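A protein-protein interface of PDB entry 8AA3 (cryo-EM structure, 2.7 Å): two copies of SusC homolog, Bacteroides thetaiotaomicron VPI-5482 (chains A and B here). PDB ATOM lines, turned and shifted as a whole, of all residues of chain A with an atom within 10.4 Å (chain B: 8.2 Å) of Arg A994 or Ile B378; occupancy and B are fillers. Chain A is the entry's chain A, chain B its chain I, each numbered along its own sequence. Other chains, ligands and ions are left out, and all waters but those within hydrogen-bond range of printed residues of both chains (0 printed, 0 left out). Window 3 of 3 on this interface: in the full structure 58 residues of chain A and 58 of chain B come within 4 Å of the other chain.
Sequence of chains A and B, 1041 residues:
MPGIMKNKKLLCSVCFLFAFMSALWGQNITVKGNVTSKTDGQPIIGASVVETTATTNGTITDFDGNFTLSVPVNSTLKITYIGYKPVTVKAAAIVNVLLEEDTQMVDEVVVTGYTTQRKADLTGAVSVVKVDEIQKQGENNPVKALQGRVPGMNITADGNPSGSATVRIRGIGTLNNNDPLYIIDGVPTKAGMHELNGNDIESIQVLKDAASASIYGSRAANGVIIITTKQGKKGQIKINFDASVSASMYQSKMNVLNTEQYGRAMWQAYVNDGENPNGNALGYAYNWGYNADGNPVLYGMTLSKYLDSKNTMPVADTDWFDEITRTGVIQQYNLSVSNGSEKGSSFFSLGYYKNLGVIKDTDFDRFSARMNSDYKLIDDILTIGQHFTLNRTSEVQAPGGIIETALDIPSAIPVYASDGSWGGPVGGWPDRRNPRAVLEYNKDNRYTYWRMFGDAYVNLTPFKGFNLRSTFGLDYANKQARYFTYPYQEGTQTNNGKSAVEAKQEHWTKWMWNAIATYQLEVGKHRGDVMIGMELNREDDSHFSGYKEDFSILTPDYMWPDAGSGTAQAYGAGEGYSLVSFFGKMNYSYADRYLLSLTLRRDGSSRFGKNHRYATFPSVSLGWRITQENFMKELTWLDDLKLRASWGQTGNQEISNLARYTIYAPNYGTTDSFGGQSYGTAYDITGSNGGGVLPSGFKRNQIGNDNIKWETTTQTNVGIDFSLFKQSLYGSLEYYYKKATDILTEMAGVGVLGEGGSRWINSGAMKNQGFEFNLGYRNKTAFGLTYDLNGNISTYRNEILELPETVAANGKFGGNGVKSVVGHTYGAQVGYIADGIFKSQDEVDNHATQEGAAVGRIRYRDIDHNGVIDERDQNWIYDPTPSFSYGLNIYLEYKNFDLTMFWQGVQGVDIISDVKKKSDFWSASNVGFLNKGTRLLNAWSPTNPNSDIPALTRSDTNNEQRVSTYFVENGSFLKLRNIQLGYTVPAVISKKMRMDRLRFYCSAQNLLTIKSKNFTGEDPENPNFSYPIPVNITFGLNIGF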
ATOM      1  N   ILE A 237      20.852 -19.678   2.639  1.00  0.00           N
ATOM      2  CA  ILE A 237      20.422 -18.313   2.912  1.00  0.00           C
ATOM      3  C   ILE A 237      21.553 -17.375   2.506  1.00  0.00           C
ATOM      4  O   ILE A 237      22.711 -17.594   2.876  1.00  0.00           O
ATOM      5  CB  ILE A 237      20.034 -18.127   4.394  1.00  0.00           C
ATOM      6  CG1 ILE A 237      19.643 -16.679   4.688  1.00  0.00           C
ATOM      7  CG2 ILE A 237      21.146 -18.610   5.323  1.00  0.00           C
ATOM      8  CD1 ILE A 237      18.739 -16.543   5.894  1.00  0.00           C
ATOM      9  N   LYS A 238      21.222 -16.346   1.726  1.00  0.00           N
ATOM     10  CA  LYS A 238      22.233 -15.485   1.124  1.00  0.00           C
ATOM     11  C   LYS A 238      21.772 -14.034   1.134  1.00  0.00           C
ATOM     12  O   LYS A 238      20.584 -13.734   1.273  1.00  0.00           O
ATOM     13  CB  LYS A 238      22.555 -15.914  -0.316  1.00  0.00           C
ATOM     14  CG  LYS A 238      23.247 -17.262  -0.435  1.00  0.00           C
ATOM     15  CD  LYS A 238      23.717 -17.514  -1.858  1.00  0.00           C
ATOM     16  CE  LYS A 238      22.542 -17.775  -2.786  1.00  0.00           C
ATOM     17  NZ  LYS A 238      22.985 -18.120  -4.165  1.00  0.00           N
ATOM     18  N   ILE A 239      22.745 -13.133   0.979  1.00  0.00           N
ATOM     19  CA  ILE A 239      22.499 -11.700   0.880  1.00  0.00           C
ATOM     20  C   ILE A 239      23.460 -11.115  -0.147  1.00  0.00           C
ATOM     21  O   ILE A 239      24.585 -11.594  -0.319  1.00  0.00           O
ATOM     22  CB  ILE A 239      22.652 -10.989   2.246  1.00  0.00           C
ATOM     23  CG1 ILE A 239      22.203  -9.528   2.162  1.00  0.00           C
ATOM     24  CG2 ILE A 239      24.084 -11.066   2.738  1.00  0.00           C
ATOM     25  CD1 ILE A 239      22.180  -8.825   3.497  1.00  0.00           C
ATOM     26  N   ASN A 240      23.000 -10.080  -0.847  1.00  0.00           N
ATOM     27  CA  ASN A 240      23.810  -9.381  -1.837  1.00  0.00           C
ATOM     28  C   ASN A 240      23.541  -7.888  -1.742  1.00  0.00           C
ATOM     29  O   ASN A 240      22.385  -7.457  -1.804  1.00  0.00           O
ATOM     30  CB  ASN A 240      23.510  -9.884  -3.255  1.00  0.00           C
ATOM     31  CG  ASN A 240      24.119 -11.244  -3.531  1.00  0.00           C
ATOM     32  OD1 ASN A 240      23.584 -12.273  -3.118  1.00  0.00           O
ATOM     33  ND2 ASN A 240      25.247 -11.256  -4.234  1.00  0.00           N
ATOM     34  N   VAL A 337      18.009 -10.205   0.004  1.00  0.00           N
ATOM     35  CA  VAL A 337      18.241 -11.330   0.901  1.00  0.00           C
ATOM     36  C   VAL A 337      17.281 -12.451   0.525  1.00  0.00           C
ATOM     37  O   VAL A 337      16.117 -12.203   0.195  1.00  0.00           O
ATOM     38  CB  VAL A 337      18.087 -10.920   2.382  1.00  0.00           C
ATOM     39  CG1 VAL A 337      16.659 -10.483   2.686  1.00  0.00           C
ATOM     40  CG2 VAL A 337      18.514 -12.054   3.302  1.00  0.00           C
ATOM     41  N   SER A 338      17.780 -13.684   0.542  1.00  0.00           N
ATOM     42  CA  SER A 338      16.975 -14.848   0.204  1.00  0.00           C
ATOM     43  C   SER A 338      17.233 -15.947   1.223  1.00  0.00           C
ATOM     44  O   SER A 338      18.336 -16.065   1.762  1.00  0.00           O
ATOM     45  CB  SER A 338      17.282 -15.359  -1.210  1.00  0.00           C
ATOM     46  OG  SER A 338      18.582 -15.919  -1.279  1.00  0.00           O
ATOM     47  N   VAL A 985      37.822 -10.214  -5.195  1.00  0.00           N
ATOM     48  CA  VAL A 985      38.723 -10.527  -4.081  1.00  0.00           C
ATOM     49  C   VAL A 985      38.920 -12.035  -4.008  1.00  0.00           C
ATOM     50  O   VAL A 985      37.938 -12.794  -4.144  1.00  0.00           O
ATOM     51  CB  VAL A 985      38.157  -9.977  -2.760  1.00  0.00           C
ATOM     52  CG1 VAL A 985      38.945 -10.504  -1.569  1.00  0.00           C
ATOM     53  CG2 VAL A 985      38.166  -8.457  -2.776  1.00  0.00           C
ATOM     54  N   PRO A 986      40.144 -12.529  -3.818  1.00  0.00           N
ATOM     55  CA  PRO A 986      40.348 -13.980  -3.731  1.00  0.00           C
ATOM     56  C   PRO A 986      39.592 -14.582  -2.555  1.00  0.00           C
ATOM     57  O   PRO A 986      39.312 -13.914  -1.558  1.00  0.00           O
ATOM     58  CB  PRO A 986      41.864 -14.117  -3.554  1.00  0.00           C
ATOM     59  CG  PRO A 986      42.427 -12.859  -4.130  1.00  0.00           C
ATOM     60  CD  PRO A 986      41.418 -11.790  -3.829  1.00  0.00           C
ATOM     61  N   ALA A 987      39.256 -15.866  -2.696  1.00  0.00           N
ATOM     62  CA  ALA A 987      38.370 -16.522  -1.738  1.00  0.00           C
ATOM     63  C   ALA A 987      38.960 -16.534  -0.334  1.00  0.00           C
ATOM     64  O   ALA A 987      38.224 -16.429   0.653  1.00  0.00           O
ATOM     65  CB  ALA A 987      38.061 -17.945  -2.202  1.00  0.00           C
ATOM     66  N   VAL A 988      40.283 -16.672  -0.217  1.00  0.00           N
ATOM     67  CA  VAL A 988      40.893 -16.775   1.106  1.00  0.00           C
ATOM     68  C   VAL A 988      40.789 -15.451   1.861  1.00  0.00           C
ATOM     69  O   VAL A 988      40.487 -15.432   3.062  1.00  0.00           O
ATOM     70  CB  VAL A 988      42.347 -17.276   0.993  1.00  0.00           C
ATOM     71  CG1 VAL A 988      43.198 -16.330   0.161  1.00  0.00           C
ATOM     72  CG2 VAL A 988      42.952 -17.467   2.377  1.00  0.00           C
ATOM     73  N   ILE A 989      41.014 -14.324   1.177  1.00  0.00           N
ATOM     74  CA  ILE A 989      40.858 -13.027   1.830  1.00  0.00           C
ATOM     75  C   ILE A 989      39.402 -12.798   2.219  1.00  0.00           C
ATOM     76  O   ILE A 989      39.108 -12.291   3.310  1.00  0.00           O
ATOM     77  CB  ILE A 989      41.389 -11.889   0.936  1.00  0.00           C
ATOM     78  CG1 ILE A 989      42.898 -12.019   0.702  1.00  0.00           C
ATOM     79  CG2 ILE A 989      41.069 -10.531   1.544  1.00  0.00           C
ATOM     80  CD1 ILE A 989      43.282 -12.832  -0.509  1.00  0.00           C
ATOM     81  N   SER A 990      38.468 -13.166   1.337  1.00  0.00           N
ATOM     82  CA  SER A 990      37.052 -12.992   1.642  1.00  0.00           C
ATOM     83  C   SER A 990      36.640 -13.820   2.853  1.00  0.00           C
ATOM     84  O   SER A 990      35.880 -13.349   3.707  1.00  0.00           O
ATOM     85  CB  SER A 990      36.208 -13.362   0.422  1.00  0.00           C
ATOM     86  OG  SER A 990      36.168 -14.765   0.235  1.00  0.00           O
ATOM     87  N   LYS A 991      37.131 -15.058   2.945  1.00  0.00           N
ATOM     88  CA  LYS A 991      36.849 -15.883   4.115  1.00  0.00           C
ATOM     89  C   LYS A 991      37.503 -15.319   5.369  1.00  0.00           C
ATOM     90  O   LYS A 991      36.940 -15.432   6.464  1.00  0.00           O
ATOM     91  CB  LYS A 991      37.310 -17.320   3.873  1.00  0.00           C
ATOM     92  CG  LYS A 991      36.500 -18.062   2.823  1.00  0.00           C
ATOM     93  CD  LYS A 991      35.111 -18.408   3.337  1.00  0.00           C
ATOM     94  CE  LYS A 991      34.388 -19.346   2.385  1.00  0.00           C
ATOM     95  NZ  LYS A 991      33.005 -18.879   2.089  1.00  0.00           N
ATOM     96  N   LYS A 992      38.689 -14.719   5.233  1.00  0.00           N
ATOM     97  CA  LYS A 992      39.305 -14.039   6.368  1.00  0.00           C
ATOM     98  C   LYS A 992      38.434 -12.887   6.852  1.00  0.00           C
ATOM     99  O   LYS A 992      38.300 -12.662   8.060  1.00  0.00           O
ATOM    100  CB  LYS A 992      40.699 -13.540   5.990  1.00  0.00           C
ATOM    101  CG  LYS A 992      41.434 -12.834   7.118  1.00  0.00           C
ATOM    102  CD  LYS A 992      42.830 -12.410   6.689  1.00  0.00           C
ATOM    103  CE  LYS A 992      42.780 -11.216   5.750  1.00  0.00           C
ATOM    104  NZ  LYS A 992      44.142 -10.711   5.422  1.00  0.00           N
ATOM    105  N   MET A 993      37.832 -12.149   5.922  1.00  0.00           N
ATOM    106  CA  MET A 993      36.879 -11.099   6.251  1.00  0.00           C
ATOM    107  C   MET A 993      35.456 -11.623   6.386  1.00  0.00           C
ATOM    108  O   MET A 993      34.530 -10.818   6.538  1.00  0.00           O
ATOM    109  CB  MET A 993      36.922  -9.992   5.193  1.00  0.00           C
ATOM    110  CG  MET A 993      38.324  -9.528   4.834  1.00  0.00           C
ATOM    111  SD  MET A 993      38.325  -8.100   3.733  1.00  0.00           S
ATOM    112  CE  MET A 993      37.432  -6.907   4.727  1.00  0.00           C
ATOM    113  N   ARG A 994      35.264 -12.942   6.288  1.00  0.00           N
ATOM    114  CA  ARG A 994      33.987 -13.621   6.508  1.00  0.00           C
ATOM    115  C   ARG A 994      33.025 -13.356   5.350  1.00  0.00           C
ATOM    116  O   ARG A 994      31.936 -13.936   5.291  1.00  0.00           O
ATOM    117  CB  ARG A 994      33.384 -13.199   7.855  1.00  0.00           C
ATOM    118  CG  ARG A 994      32.141 -13.962   8.289  1.00  0.00           C
ATOM    119  CD  ARG A 994      31.654 -13.487   9.647  1.00  0.00           C
ATOM    120  NE  ARG A 994      32.620 -13.768  10.703  1.00  0.00           N
ATOM    121  CZ  ARG A 994      33.288 -12.839  11.373  1.00  0.00           C
ATOM    122  NH1 ARG A 994      33.120 -11.551  11.124  1.00  0.00           N
ATOM    123  NH2 ARG A 994      34.147 -13.211  12.319  1.00  0.00           N
ATOM    124  N   MET A 995      33.429 -12.506   4.412  1.00  0.00           N
ATOM    125  CA  MET A 995      32.607 -12.235   3.241  1.00  0.00           C
ATOM    126  C   MET A 995      32.600 -13.441   2.308  1.00  0.00           C
ATOM    127  O   MET A 995      33.630 -14.084   2.090  1.00  0.00           O
ATOM    128  CB  MET A 995      33.131 -11.006   2.499  1.00  0.00           C
ATOM    129  CG  MET A 995      33.084  -9.719   3.306  1.00  0.00           C
ATOM    130  SD  MET A 995      33.752  -8.317   2.391  1.00  0.00           S
ATOM    131  CE  MET A 995      33.723  -7.039   3.646  1.00  0.00           C
ATOM    132  N   ASP A 996      31.423 -13.757   1.764  1.00  0.00           N
ATOM    133  CA  ASP A 996      31.346 -14.819   0.768  1.00  0.00           C
ATOM    134  C   ASP A 996      31.831 -14.355  -0.599  1.00  0.00           C
ATOM    135  O   ASP A 996      32.403 -15.151  -1.352  1.00  0.00           O
ATOM    136  CB  ASP A 996      29.915 -15.351   0.666  1.00  0.00           C
ATOM    137  N   ARG A 997      31.616 -13.083  -0.936  1.00  0.00           N
ATOM    138  CA  ARG A 997      32.055 -12.548  -2.219  1.00  0.00           C
ATOM    139  C   ARG A 997      32.218 -11.040  -2.098  1.00  0.00           C
ATOM    140  O   ARG A 997      31.353 -10.365  -1.534  1.00  0.00           O
ATOM    141  CB  ARG A 997      31.055 -12.887  -3.331  1.00  0.00           C
ATOM    142  CG  ARG A 997      31.511 -12.467  -4.720  1.00  0.00           C
ATOM    143  CD  ARG A 997      30.851 -13.308  -5.800  1.00  0.00           C
ATOM    144  NE  ARG A 997      30.643 -12.552  -7.029  1.00  0.00           N
ATOM    145  CZ  ARG A 997      29.650 -11.696  -7.224  1.00  0.00           C
ATOM    146  NH1 ARG A 997      28.744 -11.461  -6.289  1.00  0.00           N
ATOM    147  NH2 ARG A 997      29.561 -11.060  -8.390  1.00  0.00           N
ATOM    148  N   LEU A 998      33.325 -10.523  -2.629  1.00  0.00           N
ATOM    149  CA  LEU A 998      33.585  -9.087  -2.667  1.00  0.00           C
ATOM    150  C   LEU A 998      34.193  -8.754  -4.019  1.00  0.00           C
ATOM    151  O   LEU A 998      35.279  -9.242  -4.348  1.00  0.00           O
ATOM    152  CB  LEU A 998      34.522  -8.658  -1.533  1.00  0.00           C
ATOM    153  CG  LEU A 998      34.936  -7.184  -1.514  1.00  0.00           C
ATOM    154  CD1 LEU A 998      33.722  -6.273  -1.622  1.00  0.00           C
ATOM    155  CD2 LEU A 998      35.747  -6.863  -0.266  1.00  0.00           C
ATOM    156  N   ILE A1039      28.944  -6.906  -2.585  1.00  0.00           N
ATOM    157  CA  ILE A1039      29.306  -7.542  -1.325  1.00  0.00           C
ATOM    158  C   ILE A1039      28.336  -8.687  -1.073  1.00  0.00           C
ATOM    159  O   ILE A1039      27.121  -8.525  -1.235  1.00  0.00           O
ATOM    160  CB  ILE A1039      29.284  -6.538  -0.157  1.00  0.00           C
ATOM    161  CG1 ILE A1039      30.333  -5.445  -0.371  1.00  0.00           C
ATOM    162  CG2 ILE A1039      29.524  -7.245   1.165  1.00  0.00           C
ATOM    163  CD1 ILE A1039      30.163  -4.249   0.539  1.00  0.00           C
ATOM    164  N   GLY A1040      28.872  -9.840  -0.683  1.00  0.00           N
ATOM    165  CA  GLY A1040      28.064 -11.019  -0.451  1.00  0.00           C
ATOM    166  C   GLY A1040      28.108 -11.530   0.976  1.00  0.00           C
ATOM    167  O   GLY A1040      28.366 -12.715   1.196  1.00  0.00           O
ATOM    168  N   PHE A1041      27.883 -10.645   1.946  1.00  0.00           N
ATOM    169  CA  PHE A1041      27.867 -11.006   3.367  1.00  0.00           C
ATOM    170  C   PHE A1041      27.102 -12.296   3.656  1.00  0.00           C
ATOM    171  O   PHE A1041      27.696 -13.328   3.966  1.00  0.00           O
ATOM    172  CB  PHE A1041      27.263  -9.870   4.196  1.00  0.00           C
ATOM    173  CG  PHE A1041      28.175  -8.690   4.370  1.00  0.00           C
ATOM    174  CD1 PHE A1041      29.548  -8.856   4.399  1.00  0.00           C
ATOM    175  CD2 PHE A1041      27.656  -7.413   4.505  1.00  0.00           C
ATOM    176  CE1 PHE A1041      30.387  -7.771   4.563  1.00  0.00           C
ATOM    177  CE2 PHE A1041      28.490  -6.324   4.667  1.00  0.00           C
ATOM    178  CZ  PHE A1041      29.857  -6.503   4.696  1.00  0.00           C
ATOM    179  N   LYS B 343      16.839 -20.247  10.325  1.00  0.00           N
ATOM    180  CA  LYS B 343      17.455 -19.169   9.564  1.00  0.00           C
ATOM    181  C   LYS B 343      16.498 -18.019   9.277  1.00  0.00           C
ATOM    182  O   LYS B 343      16.918 -17.017   8.689  1.00  0.00           O
ATOM    183  CB  LYS B 343      18.018 -19.709   8.246  1.00  0.00           C
ATOM    184  CG  LYS B 343      19.016 -20.842   8.417  1.00  0.00           C
ATOM    185  CD  LYS B 343      20.356 -20.326   8.915  1.00  0.00           C
ATOM    186  CE  LYS B 343      21.490 -21.251   8.508  1.00  0.00           C
ATOM    187  NZ  LYS B 343      22.788 -20.528   8.404  1.00  0.00           N
ATOM    188  N   TYR B 375      14.948 -12.685   8.451  1.00  0.00           N
ATOM    189  CA  TYR B 375      16.073 -13.520   8.060  1.00  0.00           C
ATOM    190  C   TYR B 375      17.230 -13.273   9.016  1.00  0.00           C
ATOM    191  O   TYR B 375      17.516 -12.124   9.371  1.00  0.00           O
ATOM    192  CB  TYR B 375      16.525 -13.223   6.622  1.00  0.00           C
ATOM    193  CG  TYR B 375      15.398 -13.004   5.635  1.00  0.00           C
ATOM    194  CD1 TYR B 375      14.795 -11.759   5.504  1.00  0.00           C
ATOM    195  CD2 TYR B 375      14.946 -14.037   4.828  1.00  0.00           C
ATOM    196  CE1 TYR B 375      13.768 -11.554   4.603  1.00  0.00           C
ATOM    197  CE2 TYR B 375      13.921 -13.841   3.922  1.00  0.00           C
ATOM    198  CZ  TYR B 375      13.335 -12.598   3.814  1.00  0.00           C
ATOM    199  OH  TYR B 375      12.314 -12.398   2.915  1.00  0.00           O
ATOM    200  N   LYS B 376      17.893 -14.351   9.424  1.00  0.00           N
ATOM    201  CA  LYS B 376      19.060 -14.281  10.295  1.00  0.00           C
ATOM    202  C   LYS B 376      20.272 -14.776   9.520  1.00  0.00           C
ATOM    203  O   LYS B 376      20.284 -15.917   9.046  1.00  0.00           O
ATOM    204  CB  LYS B 376      18.851 -15.110  11.564  1.00  0.00           C
ATOM    205  CG  LYS B 376      17.705 -14.628  12.437  1.00  0.00           C
ATOM    206  CD  LYS B 376      17.535 -15.505  13.666  1.00  0.00           C
ATOM    207  CE  LYS B 376      16.441 -14.972  14.576  1.00  0.00           C
ATOM    208  NZ  LYS B 376      15.100 -15.056  13.937  1.00  0.00           N
ATOM    209  N   LEU B 377      21.284 -13.921   9.393  1.00  0.00           N
ATOM    210  CA  LEU B 377      22.493 -14.237   8.650  1.00  0.00           C
ATOM    211  C   LEU B 377      23.709 -13.936   9.514  1.00  0.00           C
ATOM    212  O   LEU B 377      23.627 -13.216  10.516  1.00  0.00           O
ATOM    213  CB  LEU B 377      22.582 -13.443   7.337  1.00  0.00           C
ATOM    214  CG  LEU B 377      21.680 -13.853   6.171  1.00  0.00           C
ATOM    215  CD1 LEU B 377      20.249 -13.376   6.388  1.00  0.00           C
ATOM    216  CD2 LEU B 377      22.230 -13.350   4.854  1.00  0.00           C
ATOM    217  N   ILE B 378      24.850 -14.485   9.093  1.00  0.00           N
ATOM    218  CA  ILE B 378      26.118 -14.357   9.807  1.00  0.00           C
ATOM    219  C   ILE B 378      25.924 -14.821  11.243  1.00  0.00           C
ATOM    220  O   ILE B 378      25.863 -13.998  12.163  1.00  0.00           O
ATOM    221  CB  ILE B 378      26.655 -12.915   9.755  1.00  0.00           C
ATOM    222  CG1 ILE B 378      26.474 -12.321   8.354  1.00  0.00           C
ATOM    223  CG2 ILE B 378      28.118 -12.874  10.162  1.00  0.00           C
ATOM    224  CD1 ILE B 378      27.256 -13.040   7.278  1.00  0.00           C
ATOM    225  N   ASP B 379      25.750 -16.137  11.418  1.00  0.00           N
ATOM    226  CA  ASP B 379      25.608 -16.850  12.692  1.00  0.00           C
ATOM    227  C   ASP B 379      24.904 -16.013  13.758  1.00  0.00           C
ATOM    228  O   ASP B 379      25.425 -15.822  14.862  1.00  0.00           O
ATOM    229  CB  ASP B 379      26.961 -17.407  13.189  1.00  0.00           C
ATOM    230  CG  ASP B 379      27.992 -16.340  13.549  1.00  0.00           C
ATOM    231  OD1 ASP B 379      27.737 -15.133  13.424  1.00  0.00           O
ATOM    232  OD2 ASP B 379      29.099 -16.735  13.972  1.00  0.00           O
ATOM    233  N   ASP B 380      23.714 -15.513  13.419  1.00  0.00           N
ATOM    234  CA  ASP B 380      22.803 -14.752  14.272  1.00  0.00           C
ATOM    235  C   ASP B 380      23.292 -13.343  14.587  1.00  0.00           C
ATOM    236  O   ASP B 380      22.626 -12.636  15.353  1.00  0.00           O
ATOM    237  CB  ASP B 380      22.496 -15.475  15.593  1.00  0.00           C
ATOM    238  CG  ASP B 380      21.443 -16.554  15.436  1.00  0.00           C
ATOM    239  OD1 ASP B 380      21.360 -17.150  14.341  1.00  0.00           O
ATOM    240  OD2 ASP B 380      20.700 -16.809  16.406  1.00  0.00           O
ATOM    241  N   ILE B 381      24.424 -12.905  14.033  1.00  0.00           N
ATOM    242  CA  ILE B 381      24.863 -11.529  14.253  1.00  0.00           C
ATOM    243  C   ILE B 381      23.958 -10.554  13.509  1.00  0.00           C
ATOM    244  O   ILE B 381      23.538  -9.530  14.060  1.00  0.00           O
ATOM    245  CB  ILE B 381      26.338 -11.353  13.843  1.00  0.00           C
ATOM    246  CG1 ILE B 381      27.252 -12.178  14.749  1.00  0.00           C
ATOM    247  CG2 ILE B 381      26.733  -9.885  13.872  1.00  0.00           C
ATOM    248  CD1 ILE B 381      28.690 -12.233  14.274  1.00  0.00           C
ATOM    249  N   LEU B 382      23.639 -10.856  12.254  1.00  0.00           N
ATOM    250  CA  LEU B 382      22.857  -9.958  11.416  1.00  0.00           C
ATOM    251  C   LEU B 382      21.425 -10.460  11.294  1.00  0.00           C
ATOM    252  O   LEU B 382      21.188 -11.663  11.157  1.00  0.00           O
ATOM    253  CB  LEU B 382      23.485  -9.827  10.027  1.00  0.00           C
ATOM    254  CG  LEU B 382      22.810  -8.854   9.057  1.00  0.00           C
ATOM    255  CD1 LEU B 382      22.867  -7.433   9.596  1.00  0.00           C
ATOM    256  CD2 LEU B 382      23.452  -8.935   7.681  1.00  0.00           C
ATOM    257  N   THR B 383      20.472  -9.534  11.348  1.00  0.00           N
ATOM    258  CA  THR B 383      19.066  -9.858  11.159  1.00  0.00           C
ATOM    259  C   THR B 383      18.425  -8.785  10.294  1.00  0.00           C
ATOM    260  O   THR B 383      18.686  -7.595  10.477  1.00  0.00           O
ATOM    261  CB  THR B 383      18.324  -9.963  12.499  1.00  0.00           C
ATOM    262  OG1 THR B 383      19.117 -10.708  13.431  1.00  0.00           O
ATOM    263  CG2 THR B 383      16.983 -10.658  12.315  1.00  0.00           C
ATOM    264  N   LEU B 460      22.083  -5.563  14.179  1.00  0.00           N
ATOM    265  CA  LEU B 460      23.457  -6.043  14.200  1.00  0.00           C
ATOM    266  C   LEU B 460      23.921  -6.188  15.641  1.00  0.00           C
ATOM    267  O   LEU B 460      23.655  -5.320  16.479  1.00  0.00           O
ATOM    268  CB  LEU B 460      24.391  -5.093  13.441  1.00  0.00           C
ATOM    269  CG  LEU B 460      25.842  -5.547  13.270  1.00  0.00           C
ATOM    270  CD1 LEU B 460      25.952  -6.590  12.168  1.00  0.00           C
ATOM    271  CD2 LEU B 460      26.746  -4.360  12.983  1.00  0.00           C
ATOM    272  N   THR B 461      24.616  -7.286  15.927  1.00  0.00           N
ATOM    273  CA  THR B 461      25.132  -7.562  17.268  1.00  0.00           C
ATOM    274  C   THR B 461      26.648  -7.669  17.215  1.00  0.00           C
ATOM    275  O   THR B 461      27.185  -8.742  16.883  1.00  0.00           O
ATOM    276  CB  THR B 461      24.526  -8.844  17.837  1.00  0.00           C
ATOM    277  OG1 THR B 461      25.079  -9.978  17.159  1.00  0.00           O
ATOM    278  CG2 THR B 461      23.013  -8.844  17.666  1.00  0.00           C
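The backbone carbonyl oxygen (O) of Lys A238 lies within hydrogen-bond range of the backbone NH (N) of Ser A338 (2.9 Å). The backbone carbonyl oxygen of Lys B343 sits at hydrogen-bond distance from the backbone NH of Lys B376, at 2.9 Å. The backbone carbonyl oxygen of Leu B382 is in hydrogen-bond range of the backbone NH of Leu B377 (2.9 Å).
Lys B343 touches Ile A237. Ile A237 touches Lys B376 (CD1 to O, 3.6 Å). Ile A237 touches Leu B377 (CD1 to CD1, 3.5 Å). C of Lys A238 touches CD2 of Leu B377, at 3.8 Å. CB of Ile A239 touches CD2 of Leu B377, at 3.5 Å. Val A337 touches Tyr B375. Val A337 touches Leu B377. Ile B378 touches Arg A994 (CG2 to CD, 3.6 Å). Phe A1041 touches Ile B378.
Of the printed residues of chain B, Lys A238 touches Leu B377. Of chain B, only Ile B378 (3.6 Å) comes within 4 Å of Arg A994. Leu A998 touches none of the printed residues of chain B. Printed residues of chain B within 4 Å of Phe A1041: Ile B378. Printed residues of chain A within 4 Å of Lys B343: Ile A237 (3.4 Å). Of chain A, only Arg A994 and Phe A1041 come within 4 Å of Ile B378. No residue of chain A comes within 4 Å of Ile B381. Leu B460 touches none of the printed residues of chain A. The nearest residue of chain B that does not touch Arg A994 is Ile B381 (5.5 Å).
Hydrophobic or aromatic side chains of chain B that line the printed part of chain A: Tyr B375, Leu B377 and Ile B378.
No position is printed for both chains.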
